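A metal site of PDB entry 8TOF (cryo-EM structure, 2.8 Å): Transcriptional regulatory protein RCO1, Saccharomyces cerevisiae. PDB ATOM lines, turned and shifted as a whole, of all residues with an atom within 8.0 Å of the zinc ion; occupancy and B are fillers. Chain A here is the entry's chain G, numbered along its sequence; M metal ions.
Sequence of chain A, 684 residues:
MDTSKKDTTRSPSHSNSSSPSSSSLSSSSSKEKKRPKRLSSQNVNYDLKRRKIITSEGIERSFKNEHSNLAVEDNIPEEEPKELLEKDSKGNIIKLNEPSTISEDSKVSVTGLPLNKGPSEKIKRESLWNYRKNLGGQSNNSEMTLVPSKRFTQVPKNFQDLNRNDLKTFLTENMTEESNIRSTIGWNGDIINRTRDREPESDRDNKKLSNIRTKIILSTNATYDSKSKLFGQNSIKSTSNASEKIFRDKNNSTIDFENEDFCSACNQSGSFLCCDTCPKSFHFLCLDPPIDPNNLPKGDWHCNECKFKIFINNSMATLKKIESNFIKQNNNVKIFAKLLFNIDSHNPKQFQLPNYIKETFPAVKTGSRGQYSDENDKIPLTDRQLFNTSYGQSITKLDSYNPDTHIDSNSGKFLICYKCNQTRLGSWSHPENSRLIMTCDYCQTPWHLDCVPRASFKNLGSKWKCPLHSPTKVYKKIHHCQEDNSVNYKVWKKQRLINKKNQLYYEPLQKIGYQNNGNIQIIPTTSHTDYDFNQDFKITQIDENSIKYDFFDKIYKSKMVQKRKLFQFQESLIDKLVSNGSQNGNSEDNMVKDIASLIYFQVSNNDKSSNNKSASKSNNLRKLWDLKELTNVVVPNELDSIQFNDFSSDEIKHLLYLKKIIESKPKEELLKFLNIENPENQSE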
ATOM      1  N   ILE A 416     -16.422 -23.097 -28.746  1.00  0.00           N
ATOM      2  CA  ILE A 416     -15.811 -22.806 -27.459  1.00  0.00           C
ATOM      3  C   ILE A 416     -14.309 -23.008 -27.575  1.00  0.00           C
ATOM      4  O   ILE A 416     -13.824 -24.039 -28.045  1.00  0.00           O
ATOM      5  CB  ILE A 416     -16.410 -23.702 -26.361  1.00  0.00           C
ATOM      6  CG1 ILE A 416     -17.894 -23.356 -26.170  1.00  0.00           C
ATOM      7  CG2 ILE A 416     -15.655 -23.531 -25.060  1.00  0.00           C
ATOM      8  CD1 ILE A 416     -18.787 -24.564 -26.153  1.00  0.00           C
ATOM      9  N   CYS A 417     -13.549 -22.004 -27.135  1.00  0.00           N
ATOM     10  CA  CYS A 417     -12.093 -22.086 -27.137  1.00  0.00           C
ATOM     11  C   CYS A 417     -11.629 -23.034 -26.051  1.00  0.00           C
ATOM     12  O   CYS A 417     -12.257 -23.133 -24.988  1.00  0.00           O
ATOM     13  CB  CYS A 417     -11.447 -20.717 -26.921  1.00  0.00           C
ATOM     14  SG  CYS A 417      -9.758 -20.826 -26.281  1.00  0.00           S
ATOM     15  N   TYR A 418     -10.529 -23.743 -26.315  1.00  0.00           N
ATOM     16  CA  TYR A 418     -10.102 -24.801 -25.420  1.00  0.00           C
ATOM     17  C   TYR A 418      -9.550 -24.277 -24.105  1.00  0.00           C
ATOM     18  O   TYR A 418      -9.597 -25.003 -23.102  1.00  0.00           O
ATOM     19  CB  TYR A 418      -9.053 -25.672 -26.102  1.00  0.00           C
ATOM     20  CG  TYR A 418      -8.594 -26.833 -25.246  1.00  0.00           C
ATOM     21  CD1 TYR A 418      -7.533 -26.696 -24.374  1.00  0.00           C
ATOM     22  CD2 TYR A 418      -9.248 -28.054 -25.299  1.00  0.00           C
ATOM     23  CE1 TYR A 418      -7.117 -27.747 -23.584  1.00  0.00           C
ATOM     24  CE2 TYR A 418      -8.843 -29.110 -24.516  1.00  0.00           C
ATOM     25  CZ  TYR A 418      -7.778 -28.948 -23.662  1.00  0.00           C
ATOM     26  OH  TYR A 418      -7.373 -30.004 -22.879  1.00  0.00           O
ATOM     27  N   LYS A 419      -9.039 -23.053 -24.064  1.00  0.00           N
ATOM     28  CA  LYS A 419      -8.388 -22.535 -22.865  1.00  0.00           C
ATOM     29  C   LYS A 419      -9.356 -21.771 -21.966  1.00  0.00           C
ATOM     30  O   LYS A 419      -9.580 -22.165 -20.822  1.00  0.00           O
ATOM     31  CB  LYS A 419      -7.206 -21.640 -23.246  1.00  0.00           C
ATOM     32  CG  LYS A 419      -5.949 -21.946 -22.453  1.00  0.00           C
ATOM     33  CD  LYS A 419      -4.800 -21.025 -22.826  1.00  0.00           C
ATOM     34  CE  LYS A 419      -3.468 -21.619 -22.421  1.00  0.00           C
ATOM     35  NZ  LYS A 419      -3.547 -22.335 -21.118  1.00  0.00           N
ATOM     36  N   CYS A 420      -9.937 -20.667 -22.462  1.00  0.00           N
ATOM     37  CA  CYS A 420     -10.865 -19.907 -21.635  1.00  0.00           C
ATOM     38  C   CYS A 420     -12.150 -20.700 -21.408  1.00  0.00           C
ATOM     39  O   CYS A 420     -12.823 -20.532 -20.390  1.00  0.00           O
ATOM     40  CB  CYS A 420     -11.164 -18.555 -22.270  1.00  0.00           C
ATOM     41  SG  CYS A 420     -11.573 -18.583 -24.014  1.00  0.00           S
ATOM     42  N   ASN A 421     -12.481 -21.581 -22.349  1.00  0.00           N
ATOM     43  CA  ASN A 421     -13.640 -22.459 -22.202  1.00  0.00           C
ATOM     44  C   ASN A 421     -14.938 -21.684 -22.353  1.00  0.00           C
ATOM     45  O   ASN A 421     -15.956 -22.039 -21.738  1.00  0.00           O
ATOM     46  CB  ASN A 421     -13.600 -23.171 -20.854  1.00  0.00           C
ATOM     47  CG  ASN A 421     -14.360 -24.476 -20.856  1.00  0.00           C
ATOM     48  OD1 ASN A 421     -15.395 -24.598 -20.207  1.00  0.00           O
ATOM     49  ND2 ASN A 421     -13.852 -25.446 -21.594  1.00  0.00           N
ATOM     50  N   GLN A 422     -14.928 -20.633 -23.170  1.00  0.00           N
ATOM     51  CA  GLN A 422     -16.126 -19.845 -23.421  1.00  0.00           C
ATOM     52  C   GLN A 422     -15.975 -19.166 -24.760  1.00  0.00           C
ATOM     53  O   GLN A 422     -14.864 -18.991 -25.259  1.00  0.00           O
ATOM     54  CB  GLN A 422     -16.354 -18.824 -22.313  1.00  0.00           C
ATOM     55  CG  GLN A 422     -15.147 -17.969 -21.990  1.00  0.00           C
ATOM     56  CD  GLN A 422     -15.390 -17.018 -20.840  1.00  0.00           C
ATOM     57  OE1 GLN A 422     -16.226 -17.288 -19.973  1.00  0.00           O
ATOM     58  NE2 GLN A 422     -14.671 -15.907 -20.817  1.00  0.00           N
ATOM     59  N   THR A 423     -17.099 -18.771 -25.349  1.00  0.00           N
ATOM     60  CA  THR A 423     -17.122 -18.003 -26.579  1.00  0.00           C
ATOM     61  C   THR A 423     -17.532 -16.576 -26.276  1.00  0.00           C
ATOM     62  O   THR A 423     -18.560 -16.342 -25.624  1.00  0.00           O
ATOM     63  CB  THR A 423     -18.071 -18.626 -27.608  1.00  0.00           C
ATOM     64  OG1 THR A 423     -17.830 -20.030 -27.689  1.00  0.00           O
ATOM     65  CG2 THR A 423     -17.864 -17.990 -28.968  1.00  0.00           C
ATOM     66  N   ARG A 424     -16.744 -15.620 -26.758  1.00  0.00           N
ATOM     67  CA  ARG A 424     -16.993 -14.204 -26.528  1.00  0.00           C
ATOM     68  C   ARG A 424     -17.413 -13.568 -27.843  1.00  0.00           C
ATOM     69  O   ARG A 424     -16.654 -13.587 -28.810  1.00  0.00           O
ATOM     70  CB  ARG A 424     -15.732 -13.508 -26.003  1.00  0.00           C
ATOM     71  CG  ARG A 424     -14.831 -14.360 -25.120  1.00  0.00           C
ATOM     72  CD  ARG A 424     -15.289 -14.363 -23.689  1.00  0.00           C
ATOM     73  NE  ARG A 424     -14.797 -13.195 -22.974  1.00  0.00           N
ATOM     74  CZ  ARG A 424     -13.525 -12.992 -22.647  1.00  0.00           C
ATOM     75  NH1 ARG A 424     -12.584 -13.867 -22.950  1.00  0.00           N
ATOM     76  NH2 ARG A 424     -13.196 -11.874 -21.996  1.00  0.00           N
ATOM     77  N   ARG A 435     -14.204 -11.452 -28.725  1.00  0.00           N
ATOM     78  CA  ARG A 435     -12.813 -11.874 -28.835  1.00  0.00           C
ATOM     79  C   ARG A 435     -12.702 -12.812 -30.031  1.00  0.00           C
ATOM     80  O   ARG A 435     -13.491 -13.753 -30.148  1.00  0.00           O
ATOM     81  CB  ARG A 435     -12.327 -12.559 -27.569  1.00  0.00           C
ATOM     82  CG  ARG A 435     -12.374 -11.651 -26.360  1.00  0.00           C
ATOM     83  CD  ARG A 435     -11.021 -11.059 -26.049  1.00  0.00           C
ATOM     84  NE  ARG A 435     -11.040 -10.269 -24.826  1.00  0.00           N
ATOM     85  CZ  ARG A 435     -11.693  -9.128 -24.693  1.00  0.00           C
ATOM     86  NH1 ARG A 435     -12.352  -8.574 -25.699  1.00  0.00           N
ATOM     87  NH2 ARG A 435     -11.682  -8.505 -23.514  1.00  0.00           N
ATOM     88  N   LEU A 436     -11.740 -12.559 -30.905  1.00  0.00           N
ATOM     89  CA  LEU A 436     -11.607 -13.361 -32.107  1.00  0.00           C
ATOM     90  C   LEU A 436     -11.341 -14.816 -31.750  1.00  0.00           C
ATOM     91  O   LEU A 436     -10.664 -15.114 -30.761  1.00  0.00           O
ATOM     92  CB  LEU A 436     -10.478 -12.827 -32.980  1.00  0.00           C
ATOM     93  CG  LEU A 436     -10.602 -11.359 -33.408  1.00  0.00           C
ATOM     94  CD1 LEU A 436      -9.270 -10.879 -33.932  1.00  0.00           C
ATOM     95  CD2 LEU A 436     -11.677 -11.203 -34.462  1.00  0.00           C
ATOM     96  N   ILE A 437     -11.890 -15.713 -32.559  1.00  0.00           N
ATOM     97  CA  ILE A 437     -11.720 -17.147 -32.369  1.00  0.00           C
ATOM     98  C   ILE A 437     -11.418 -17.756 -33.727  1.00  0.00           C
ATOM     99  O   ILE A 437     -11.925 -17.308 -34.761  1.00  0.00           O
ATOM    100  CB  ILE A 437     -12.973 -17.807 -31.746  1.00  0.00           C
ATOM    101  CG1 ILE A 437     -12.563 -18.845 -30.708  1.00  0.00           C
ATOM    102  CG2 ILE A 437     -13.844 -18.439 -32.806  1.00  0.00           C
ATOM    103  CD1 ILE A 437     -13.703 -19.340 -29.876  1.00  0.00           C
ATOM    104  N   PRO A 446     -11.624 -25.010 -31.585  1.00  0.00           N
ATOM    105  CA  PRO A 446     -11.575 -23.542 -31.605  1.00  0.00           C
ATOM    106  C   PRO A 446     -10.585 -23.024 -30.575  1.00  0.00           C
ATOM    107  O   PRO A 446     -10.456 -23.561 -29.478  1.00  0.00           O
ATOM    108  CB  PRO A 446     -13.007 -23.127 -31.251  1.00  0.00           C
ATOM    109  CG  PRO A 446     -13.803 -24.389 -31.207  1.00  0.00           C
ATOM    110  CD  PRO A 446     -12.845 -25.491 -30.939  1.00  0.00           C
ATOM    111  N   TRP A 447      -9.889 -21.954 -30.940  1.00  0.00           N
ATOM    112  CA  TRP A 447      -8.991 -21.261 -30.039  1.00  0.00           C
ATOM    113  C   TRP A 447      -9.212 -19.759 -30.148  1.00  0.00           C
ATOM    114  O   TRP A 447      -9.485 -19.247 -31.231  1.00  0.00           O
ATOM    115  CB  TRP A 447      -7.519 -21.568 -30.347  1.00  0.00           C
ATOM    116  CG  TRP A 447      -7.027 -22.880 -29.817  1.00  0.00           C
ATOM    117  CD1 TRP A 447      -7.068 -24.074 -30.453  1.00  0.00           C
ATOM    118  CD2 TRP A 447      -6.425 -23.114 -28.542  1.00  0.00           C
ATOM    119  NE1 TRP A 447      -6.518 -25.051 -29.659  1.00  0.00           N
ATOM    120  CE2 TRP A 447      -6.120 -24.486 -28.474  1.00  0.00           C
ATOM    121  CE3 TRP A 447      -6.111 -22.309 -27.450  1.00  0.00           C
ATOM    122  CZ2 TRP A 447      -5.528 -25.061 -27.361  1.00  0.00           C
ATOM    123  CZ3 TRP A 447      -5.523 -22.881 -26.346  1.00  0.00           C
ATOM    124  CH2 TRP A 447      -5.236 -24.236 -26.311  1.00  0.00           C
ATOM    125  N   HIS A 448      -9.106 -19.073 -29.020  1.00  0.00           N
ATOM    126  CA  HIS A 448      -9.068 -17.624 -29.042  1.00  0.00           C
ATOM    127  C   HIS A 448      -7.700 -17.147 -29.513  1.00  0.00           C
ATOM    128  O   HIS A 448      -6.663 -17.625 -29.057  1.00  0.00           O
ATOM    129  CB  HIS A 448      -9.347 -17.040 -27.656  1.00  0.00           C
ATOM    130  CG  HIS A 448     -10.798 -16.908 -27.335  1.00  0.00           C
ATOM    131  ND1 HIS A 448     -11.407 -17.649 -26.347  1.00  0.00           N
ATOM    132  CD2 HIS A 448     -11.761 -16.130 -27.873  1.00  0.00           C
ATOM    133  CE1 HIS A 448     -12.687 -17.320 -26.291  1.00  0.00           C
ATOM    134  NE2 HIS A 448     -12.923 -16.399 -27.205  1.00  0.00           N
ATOM    135  N   LEU A 449      -7.706 -16.178 -30.423  1.00  0.00           N
ATOM    136  CA  LEU A 449      -6.448 -15.578 -30.844  1.00  0.00           C
ATOM    137  C   LEU A 449      -5.674 -15.039 -29.651  1.00  0.00           C
ATOM    138  O   LEU A 449      -4.436 -15.026 -29.690  1.00  0.00           O
ATOM    139  CB  LEU A 449      -6.708 -14.461 -31.840  1.00  0.00           C
ATOM    140  CG  LEU A 449      -6.397 -14.805 -33.297  1.00  0.00           C
ATOM    141  CD1 LEU A 449      -7.221 -15.988 -33.727  1.00  0.00           C
ATOM    142  CD2 LEU A 449      -6.680 -13.620 -34.201  1.00  0.00           C
ATOM    143  N   ASP A 450      -6.363 -14.609 -28.603  1.00  0.00           N
ATOM    144  CA  ASP A 450      -5.727 -14.103 -27.401  1.00  0.00           C
ATOM    145  C   ASP A 450      -5.356 -15.203 -26.419  1.00  0.00           C
ATOM    146  O   ASP A 450      -4.672 -14.924 -25.426  1.00  0.00           O
ATOM    147  CB  ASP A 450      -6.648 -13.098 -26.710  1.00  0.00           C
ATOM    148  CG  ASP A 450      -7.066 -11.972 -27.623  1.00  0.00           C
ATOM    149  OD1 ASP A 450      -7.012 -12.158 -28.855  1.00  0.00           O
ATOM    150  OD2 ASP A 450      -7.452 -10.896 -27.112  1.00  0.00           O
ATOM    151  N   CYS A 451      -5.774 -16.444 -26.664  1.00  0.00           N
ATOM    152  CA  CYS A 451      -5.412 -17.577 -25.809  1.00  0.00           C
ATOM    153  C   CYS A 451      -4.181 -18.302 -26.333  1.00  0.00           C
ATOM    154  O   CYS A 451      -3.248 -18.572 -25.575  1.00  0.00           O
ATOM    155  CB  CYS A 451      -6.577 -18.552 -25.685  1.00  0.00           C
ATOM    156  SG  CYS A 451      -7.838 -18.023 -24.508  1.00  0.00           S
ATOM    157  N   VAL A 452      -4.159 -18.625 -27.622  1.00  0.00           N
ATOM    158  CA  VAL A 452      -2.911 -18.941 -28.310  1.00  0.00           C
ATOM    159  C   VAL A 452      -2.376 -17.611 -28.832  1.00  0.00           C
ATOM    160  O   VAL A 452      -2.832 -17.153 -29.895  1.00  0.00           O
ATOM    161  CB  VAL A 452      -3.110 -19.970 -29.426  1.00  0.00           C
ATOM    162  CG1 VAL A 452      -4.144 -19.491 -30.444  1.00  0.00           C
ATOM    163  CG2 VAL A 452      -1.779 -20.244 -30.113  1.00  0.00           C
HETATM  164 ZN    ZN M   1      -9.823 -18.645 -25.514  1.00  0.00          ZN
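The zinc ion is bound by ND1 of His 448 (2.0 Å), SG of Cys 420 (2.3 Å), SG of Cys 451 (2.3 Å) and SG of Cys 417 (2.3 Å).
The backbone carbonyl oxygen of Gln 422 lies close to the side-chain sulfur of Cys 420 (3.5 Å). SG of Cys 417 lies close to N of Lys 419 (3.2 Å).
Within 4 Å of the zinc ion: Cys 417, Cys 420, His 448 and Cys 451.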
